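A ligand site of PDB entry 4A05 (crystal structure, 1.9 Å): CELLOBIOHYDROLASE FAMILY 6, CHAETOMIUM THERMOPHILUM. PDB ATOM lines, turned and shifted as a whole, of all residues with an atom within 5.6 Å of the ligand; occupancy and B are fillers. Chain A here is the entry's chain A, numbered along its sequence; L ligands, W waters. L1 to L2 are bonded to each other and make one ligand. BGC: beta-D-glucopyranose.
CE3 of Trp 51 touches C5 of BGC L1 (3.6 Å). NE of Arg 54 touches C6 of BGC L2, at 3.2 Å. Tyr 88 touches the ligand. CD of Pro 314 touches C6 of BGC L1, 3.4 Å away. CB of Ala 345 touches O2 of BGC L1, at 3.7 Å. Gly 346 touches the ligand. Gln 347 touches the ligand. Hydrophobic or aromatic side chains that line the ligand: Trp 51, Tyr 88, Pro 314 and Ala 345. Of the 20 residues printed, 11 come within 4 Å of the ligand. The nearest printed residue that does not touch the ligand is Ser 318 (4.2 Å).
OG of Ser 100 sits at hydrogen-bond distance from O2 of BGC L1. The side-chain carboxylate of Glu 317 is in hydrogen-bond range of an oxygen (O2) of BGC L2 (2.6 Å). An oxygen (O3) of BGC L1 lies close to the side-chain carboxylate (OD2) of Asp 53, at 3.1 Å. The side-chain amino group (NZ) of Lys 313 is in hydrogen-bond range of an oxygen (O5) of BGC L1, 2.9 Å away.
Water W2 bridges an oxygen (O3) of BGC L2 (2.6 Å) and the side-chain carboxylate (OE2) of Glu 317 (3.3 Å). Water W5 bridges an oxygen (O2) of BGC L2 (2.6 Å) and the backbone NH (N) of Trp 51 (2.8 Å). Water W3 lies within hydrogen-bond range of O1 of BGC L1 (2.7 Å), OH of Tyr 88 (3.1 Å) and OG of Ser 100 (3.3 Å). Water W4 lies within hydrogen-bond range of NH1 of Arg 328, O2 of BGC L1 and NH2 of Arg 93. Water W1 lies within hydrogen-bond range of O of Ala 345, NE2 of Gln 347 and O6 of BGC L2. Water W6 lies within hydrogen-bond range of OD2 of Asp 53, NH2 of Arg 93 and O3 of BGC L1.
The backbone carbonyl oxygen (O) of Ser 100 lies within hydrogen-bond range of the guanidinium group (NE) of Arg 93, 2.9 Å away. The backbone carbonyl oxygen (O) of Glu 317 lies close to the side-chain amino group (NZ) of Lys 313 (3.1 Å). OD1 of Asp 53 lies within salt-bridge range of NE of Arg 54 (3.2 Å). O of Asp 53 is in hydrogen-bond range of NH1 of Arg 93 (2.8 Å). NZ of Lys 313 is in salt-bridge range of OD1 of Asp 319, 3.1 Å away. The backbone NH of Gly 346 is in hydrogen-bond range of the backbone carbonyl oxygen of Ser 318. The backbone carbonyl oxygen (O) of Gln 347 sits at hydrogen-bond distance from the backbone NH (N) of Ser 318. O of Tyr 88 is in hydrogen-bond range of NH1 of Arg 93 (2.8 Å).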
ATOM      1  N   TYR A  19     -20.482   4.012   7.974  1.00  0.00           N
ATOM      2  CA  TYR A  19     -21.056   4.414   6.712  1.00  0.00           C
ATOM      3  C   TYR A  19     -21.530   3.211   5.916  1.00  0.00           C
ATOM      4  O   TYR A  19     -22.620   3.254   5.335  1.00  0.00           O
ATOM      5  CB  TYR A  19     -20.092   5.317   5.954  1.00  0.00           C
ATOM      6  CG  TYR A  19     -19.668   6.464   6.852  1.00  0.00           C
ATOM      7  CD1 TYR A  19     -20.555   7.511   7.157  1.00  0.00           C
ATOM      8  CD2 TYR A  19     -18.413   6.481   7.463  1.00  0.00           C
ATOM      9  CE1 TYR A  19     -20.186   8.551   7.994  1.00  0.00           C
ATOM     10  CE2 TYR A  19     -18.027   7.526   8.310  1.00  0.00           C
ATOM     11  CZ  TYR A  19     -18.922   8.558   8.571  1.00  0.00           C
ATOM     12  OH  TYR A  19     -18.548   9.592   9.403  1.00  0.00           O
ATOM     13  N   GLU A  23     -25.521   2.383   5.139  1.00  0.00           N
ATOM     14  CA  GLU A  23     -25.977   2.007   3.790  1.00  0.00           C
ATOM     15  C   GLU A  23     -26.820   0.733   3.822  1.00  0.00           C
ATOM     16  O   GLU A  23     -27.907   0.692   3.259  1.00  0.00           O
ATOM     17  CB  GLU A  23     -24.778   1.740   2.863  1.00  0.00           C
ATOM     18  CG  GLU A  23     -24.053   2.942   2.361  1.00  0.00           C
ATOM     19  CD  GLU A  23     -23.008   2.557   1.322  1.00  0.00           C
ATOM     20  OE1 GLU A  23     -22.119   1.736   1.649  1.00  0.00           O
ATOM     21  OE2 GLU A  23     -23.107   3.054   0.190  1.00  0.00           O
ATOM     22  N   GLN A  50     -12.693   1.600   4.304  1.00  0.00           N
ATOM     23  CA  GLN A  50     -13.436   2.821   4.021  1.00  0.00           C
ATOM     24  C   GLN A  50     -12.645   3.637   3.020  1.00  0.00           C
ATOM     25  O   GLN A  50     -11.468   3.927   3.238  1.00  0.00           O
ATOM     26  CB  GLN A  50     -13.671   3.618   5.317  1.00  0.00           C
ATOM     27  CG  GLN A  50     -14.408   4.945   5.124  1.00  0.00           C
ATOM     28  CD  GLN A  50     -14.615   5.740   6.411  1.00  0.00           C
ATOM     29  OE1 GLN A  50     -14.644   6.977   6.399  1.00  0.00           O
ATOM     30  NE2 GLN A  50     -14.753   5.060   7.515  1.00  0.00           N
ATOM     31  N   TRP A  51     -13.276   3.994   1.912  1.00  0.00           N
ATOM     32  CA  TRP A  51     -12.556   4.624   0.810  1.00  0.00           C
ATOM     33  C   TRP A  51     -12.581   6.141   0.888  1.00  0.00           C
ATOM     34  O   TRP A  51     -13.654   6.748   1.001  1.00  0.00           O
ATOM     35  CB  TRP A  51     -13.171   4.195  -0.518  1.00  0.00           C
ATOM     36  CG  TRP A  51     -12.929   2.737  -0.865  1.00  0.00           C
ATOM     37  CD1 TRP A  51     -13.265   1.655  -0.104  1.00  0.00           C
ATOM     38  CD2 TRP A  51     -12.309   2.231  -2.047  1.00  0.00           C
ATOM     39  NE1 TRP A  51     -12.903   0.501  -0.748  1.00  0.00           N
ATOM     40  CE2 TRP A  51     -12.317   0.823  -1.943  1.00  0.00           C
ATOM     41  CE3 TRP A  51     -11.764   2.819  -3.193  1.00  0.00           C
ATOM     42  CZ2 TRP A  51     -11.774  -0.013  -2.941  1.00  0.00           C
ATOM     43  CZ3 TRP A  51     -11.216   1.999  -4.188  1.00  0.00           C
ATOM     44  CH2 TRP A  51     -11.233   0.600  -4.048  1.00  0.00           C
ATOM     45  N   ASP A  53     -12.473   8.433  -1.395  1.00  0.00           N
ATOM     46  CA  ASP A  53     -12.597   8.551  -2.859  1.00  0.00           C
ATOM     47  C   ASP A  53     -12.832   9.982  -3.331  1.00  0.00           C
ATOM     48  O   ASP A  53     -12.788  10.253  -4.531  1.00  0.00           O
ATOM     49  CB  ASP A  53     -13.701   7.638  -3.380  1.00  0.00           C
ATOM     50  CG  ASP A  53     -15.087   8.124  -2.984  1.00  0.00           C
ATOM     51  OD1 ASP A  53     -15.327   8.329  -1.769  1.00  0.00           O
ATOM     52  OD2 ASP A  53     -15.929   8.300  -3.883  1.00  0.00           O
ATOM     53  N   ARG A  54     -13.079  10.883  -2.377  1.00  0.00           N
ATOM     54  CA  ARG A  54     -13.294  12.294  -2.679  1.00  0.00           C
ATOM     55  C   ARG A  54     -12.607  13.095  -1.593  1.00  0.00           C
ATOM     56  O   ARG A  54     -12.482  12.650  -0.448  1.00  0.00           O
ATOM     57  CB  ARG A  54     -14.783  12.642  -2.656  1.00  0.00           C
ATOM     58  CG  ARG A  54     -15.624  12.009  -3.759  1.00  0.00           C
ATOM     59  CD  ARG A  54     -17.053  11.917  -3.312  1.00  0.00           C
ATOM     60  NE  ARG A  54     -17.211  10.922  -2.249  1.00  0.00           N
ATOM     61  CZ  ARG A  54     -17.989  11.076  -1.180  1.00  0.00           C
ATOM     62  NH1 ARG A  54     -18.679  12.201  -1.004  1.00  0.00           N
ATOM     63  NH2 ARG A  54     -18.069  10.101  -0.277  1.00  0.00           N
ATOM     64  N   LEU A  61     -15.905  12.021   6.734  1.00  0.00           N
ATOM     65  CA  LEU A  61     -16.006  10.586   7.029  1.00  0.00           C
ATOM     66  C   LEU A  61     -14.718   9.977   7.637  1.00  0.00           C
ATOM     67  O   LEU A  61     -14.807   9.130   8.535  1.00  0.00           O
ATOM     68  CB  LEU A  61     -16.421   9.808   5.768  1.00  0.00           C
ATOM     69  CG  LEU A  61     -17.531  10.407   4.870  1.00  0.00           C
ATOM     70  CD1 LEU A  61     -17.915   9.468   3.745  1.00  0.00           C
ATOM     71  CD2 LEU A  61     -18.771  10.817   5.671  1.00  0.00           C
ATOM     72  N   TYR A  88      -7.699   6.902  -2.523  1.00  0.00           N
ATOM     73  CA  TYR A  88      -8.189   6.714  -3.883  1.00  0.00           C
ATOM     74  C   TYR A  88      -8.682   8.019  -4.530  1.00  0.00           C
ATOM     75  O   TYR A  88      -9.875   8.199  -4.806  1.00  0.00           O
ATOM     76  CB  TYR A  88      -9.299   5.655  -3.896  1.00  0.00           C
ATOM     77  CG  TYR A  88      -9.729   5.208  -5.279  1.00  0.00           C
ATOM     78  CD1 TYR A  88      -8.831   4.578  -6.154  1.00  0.00           C
ATOM     79  CD2 TYR A  88     -11.047   5.382  -5.692  1.00  0.00           C
ATOM     80  CE1 TYR A  88      -9.245   4.155  -7.425  1.00  0.00           C
ATOM     81  CE2 TYR A  88     -11.461   4.959  -6.963  1.00  0.00           C
ATOM     82  CZ  TYR A  88     -10.560   4.355  -7.813  1.00  0.00           C
ATOM     83  OH  TYR A  88     -10.995   3.952  -9.055  1.00  0.00           O
ATOM     84  N   ARG A  93      -7.700   9.858 -12.360  1.00  0.00           N
ATOM     85  CA  ARG A  93      -7.910   8.544 -11.763  1.00  0.00           C
ATOM     86  C   ARG A  93      -8.505   7.559 -12.775  1.00  0.00           C
ATOM     87  O   ARG A  93      -9.173   7.992 -13.719  1.00  0.00           O
ATOM     88  CB  ARG A  93      -8.864   8.682 -10.571  1.00  0.00           C
ATOM     89  CG  ARG A  93      -8.897   7.483  -9.618  1.00  0.00           C
ATOM     90  CD  ARG A  93      -9.761   7.816  -8.412  1.00  0.00           C
ATOM     91  NE  ARG A  93     -11.176   7.933  -8.765  1.00  0.00           N
ATOM     92  CZ  ARG A  93     -12.137   8.343  -7.921  1.00  0.00           C
ATOM     93  NH1 ARG A  93     -11.836   8.681  -6.678  1.00  0.00           N
ATOM     94  NH2 ARG A  93     -13.391   8.421  -8.341  1.00  0.00           N
ATOM     95  N   ALA A  99     -15.500   4.475 -15.731  1.00  0.00           N
ATOM     96  CA  ALA A  99     -16.500   4.305 -14.667  1.00  0.00           C
ATOM     97  C   ALA A  99     -16.167   5.013 -13.367  1.00  0.00           C
ATOM     98  O   ALA A  99     -17.065   5.483 -12.675  1.00  0.00           O
ATOM     99  CB  ALA A  99     -16.757   2.812 -14.397  1.00  0.00           C
ATOM    100  N   SER A 100     -14.869   5.085 -13.045  1.00  0.00           N
ATOM    101  CA  SER A 100     -14.425   5.660 -11.775  1.00  0.00           C
ATOM    102  C   SER A 100     -13.527   6.881 -11.930  1.00  0.00           C
ATOM    103  O   SER A 100     -12.725   7.182 -11.046  1.00  0.00           O
ATOM    104  CB  SER A 100     -13.758   4.600 -10.901  1.00  0.00           C
ATOM    105  OG  SER A 100     -14.758   3.746 -10.346  1.00  0.00           O
ATOM    106  N   LYS A 313     -12.935  -3.682  -1.390  1.00  0.00           N
ATOM    107  CA  LYS A 313     -14.118  -3.201  -2.109  1.00  0.00           C
ATOM    108  C   LYS A 313     -15.361  -3.552  -1.284  1.00  0.00           C
ATOM    109  O   LYS A 313     -15.590  -4.712  -0.953  1.00  0.00           O
ATOM    110  CB  LYS A 313     -14.204  -3.824  -3.503  1.00  0.00           C
ATOM    111  CG  LYS A 313     -15.481  -3.539  -4.295  1.00  0.00           C
ATOM    112  CD  LYS A 313     -15.549  -2.126  -4.855  1.00  0.00           C
ATOM    113  CE  LYS A 313     -16.970  -1.822  -5.339  1.00  0.00           C
ATOM    114  NZ  LYS A 313     -17.087  -0.550  -6.020  1.00  0.00           N
ATOM    115  N   PRO A 314     -16.149  -2.535  -0.910  1.00  0.00           N
ATOM    116  CA  PRO A 314     -17.354  -2.854  -0.129  1.00  0.00           C
ATOM    117  C   PRO A 314     -18.452  -3.424  -1.040  1.00  0.00           C
ATOM    118  O   PRO A 314     -18.928  -2.720  -1.939  1.00  0.00           O
ATOM    119  CB  PRO A 314     -17.772  -1.494   0.446  1.00  0.00           C
ATOM    120  CG  PRO A 314     -16.585  -0.551   0.196  1.00  0.00           C
ATOM    121  CD  PRO A 314     -15.959  -1.087  -1.071  1.00  0.00           C
ATOM    122  N   GLU A 317     -21.576  -1.701  -3.311  1.00  0.00           N
ATOM    123  CA  GLU A 317     -21.276  -0.423  -3.948  1.00  0.00           C
ATOM    124  C   GLU A 317     -20.844  -0.728  -5.366  1.00  0.00           C
ATOM    125  O   GLU A 317     -19.992  -1.584  -5.594  1.00  0.00           O
ATOM    126  CB  GLU A 317     -20.203   0.367  -3.171  1.00  0.00           C
ATOM    127  CG  GLU A 317     -20.710   0.881  -1.810  1.00  0.00           C
ATOM    128  CD  GLU A 317     -19.654   1.587  -0.977  1.00  0.00           C
ATOM    129  OE1 GLU A 317     -18.543   1.875  -1.473  1.00  0.00           O
ATOM    130  OE2 GLU A 317     -19.953   1.869   0.198  1.00  0.00           O
ATOM    131  N   SER A 318     -21.453  -0.028  -6.319  1.00  0.00           N
ATOM    132  CA  SER A 318     -21.298  -0.290  -7.739  1.00  0.00           C
ATOM    133  C   SER A 318     -19.875  -0.007  -8.230  1.00  0.00           C
ATOM    134  O   SER A 318     -19.165   0.836  -7.652  1.00  0.00           O
ATOM    135  CB  SER A 318     -22.302   0.556  -8.525  1.00  0.00           C
ATOM    136  OG  SER A 318     -22.138   0.364  -9.932  1.00  0.00           O
ATOM    137  N   ASP A 319     -19.479  -0.713  -9.282  1.00  0.00           N
ATOM    138  CA  ASP A 319     -18.196  -0.497  -9.958  1.00  0.00           C
ATOM    139  C   ASP A 319     -18.362   0.486 -11.103  1.00  0.00           C
ATOM    140  O   ASP A 319     -17.375   0.933 -11.688  1.00  0.00           O
ATOM    141  CB  ASP A 319     -17.681  -1.808 -10.545  1.00  0.00           C
ATOM    142  CG  ASP A 319     -17.292  -2.804  -9.483  1.00  0.00           C
ATOM    143  OD1 ASP A 319     -16.705  -2.388  -8.473  1.00  0.00           O
ATOM    144  OD2 ASP A 319     -17.580  -4.005  -9.662  1.00  0.00           O
ATOM    145  N   ARG A 328     -19.698   8.896 -17.290  1.00  0.00           N
ATOM    146  CA  ARG A 328     -18.790   7.839 -16.833  1.00  0.00           C
ATOM    147  C   ARG A 328     -19.193   6.452 -17.336  1.00  0.00           C
ATOM    148  O   ARG A 328     -18.794   5.456 -16.739  1.00  0.00           O
ATOM    149  CB  ARG A 328     -18.699   7.831 -15.299  1.00  0.00           C
ATOM    150  CG  ARG A 328     -18.168   9.133 -14.705  1.00  0.00           C
ATOM    151  CD  ARG A 328     -17.494   8.899 -13.367  1.00  0.00           C
ATOM    152  NE  ARG A 328     -18.382   8.302 -12.362  1.00  0.00           N
ATOM    153  CZ  ARG A 328     -18.015   8.021 -11.122  1.00  0.00           C
ATOM    154  NH1 ARG A 328     -16.783   8.300 -10.714  1.00  0.00           N
ATOM    155  NH2 ARG A 328     -18.873   7.456 -10.277  1.00  0.00           N
ATOM    156  N   ALA A 345     -20.577   4.349 -10.108  1.00  0.00           N
ATOM    157  CA  ALA A 345     -19.562   3.723  -9.260  1.00  0.00           C
ATOM    158  C   ALA A 345     -19.625   4.322  -7.857  1.00  0.00           C
ATOM    159  O   ALA A 345     -19.730   5.546  -7.717  1.00  0.00           O
ATOM    160  CB  ALA A 345     -18.185   3.911  -9.855  1.00  0.00           C
ATOM    161  N   GLY A 346     -19.559   3.470  -6.853  1.00  0.00           N
ATOM    162  CA  GLY A 346     -19.607   3.917  -5.466  1.00  0.00           C
ATOM    163  C   GLY A 346     -21.009   3.987  -4.869  1.00  0.00           C
ATOM    164  O   GLY A 346     -21.171   3.830  -3.659  1.00  0.00           O
ATOM    165  N   GLN A 347     -22.010   4.236  -5.724  1.00  0.00           N
ATOM    166  CA  GLN A 347     -23.413   4.293  -5.295  1.00  0.00           C
ATOM    167  C   GLN A 347     -23.952   2.923  -4.951  1.00  0.00           C
ATOM    168  O   GLN A 347     -23.534   1.919  -5.535  1.00  0.00           O
ATOM    169  CB  GLN A 347     -24.302   4.940  -6.372  1.00  0.00           C
ATOM    170  CG  GLN A 347     -23.989   6.401  -6.644  1.00  0.00           C
ATOM    171  CD  GLN A 347     -23.958   7.215  -5.376  1.00  0.00           C
ATOM    172  OE1 GLN A 347     -24.886   7.134  -4.561  1.00  0.00           O
ATOM    173  NE2 GLN A 347     -22.910   7.991  -5.187  1.00  0.00           N
HETATM  174  C2  BGC L   1     -15.616   3.787  -6.827  1.00  0.00           C
HETATM  175  C3  BGC L   1     -15.524   4.597  -5.519  1.00  0.00           C
HETATM  176  C4  BGC L   1     -16.011   3.738  -4.366  1.00  0.00           C
HETATM  177  C5  BGC L   1     -15.214   2.439  -4.302  1.00  0.00           C
HETATM  178  C6  BGC L   1     -15.734   1.499  -3.222  1.00  0.00           C
HETATM  179  C1  BGC L   1     -14.836   2.485  -6.684  1.00  0.00           C
HETATM  180  O1  BGC L   1     -15.047   1.689  -7.839  1.00  0.00           O
HETATM  181  O2  BGC L   1     -15.103   4.556  -7.918  1.00  0.00           O
HETATM  182  O3  BGC L   1     -16.360   5.752  -5.635  1.00  0.00           O
HETATM  183  O4  BGC L   1     -15.966   4.472  -3.130  1.00  0.00           O
HETATM  184  O5  BGC L   1     -15.330   1.746  -5.559  1.00  0.00           O
HETATM  185  O6  BGC L   1     -17.062   1.103  -3.584  1.00  0.00           O
HETATM  186  C2  BGC L   2     -17.199   4.958  -1.120  1.00  0.00           C
HETATM  187  C3  BGC L   2     -18.543   5.426  -0.574  1.00  0.00           C
HETATM  188  C4  BGC L   2     -18.985   6.711  -1.242  1.00  0.00           C
HETATM  189  C5  BGC L   2     -18.884   6.687  -2.771  1.00  0.00           C
HETATM  190  C6  BGC L   2     -18.659   8.154  -3.144  1.00  0.00           C
HETATM  191  C1  BGC L   2     -17.277   4.782  -2.630  1.00  0.00           C
HETATM  192  O2  BGC L   2     -16.842   3.693  -0.569  1.00  0.00           O
HETATM  193  O3  BGC L   2     -18.402   5.726   0.817  1.00  0.00           O
HETATM  194  O4  BGC L   2     -20.346   7.015  -0.888  1.00  0.00           O
HETATM  195  O5  BGC L   2     -17.759   5.966  -3.279  1.00  0.00           O
HETATM  196  O6  BGC L   2     -19.363   8.487  -4.323  1.00  0.00           O
HETATM  197  O   HOH W   1     -20.726   7.834  -7.297  1.00  0.00           O
HETATM  198  O   HOH W   2     -19.808   4.295   2.424  1.00  0.00           O
HETATM  199  O   HOH W   3     -12.699   1.422  -9.120  1.00  0.00           O
HETATM  200  O   HOH W   4     -16.442   7.123  -8.295  1.00  0.00           O
HETATM  201  O   HOH W   5     -16.091   3.622   1.912  1.00  0.00           O
HETATM  202  O   HOH W   6     -15.389   8.993  -6.445  1.00  0.00           O
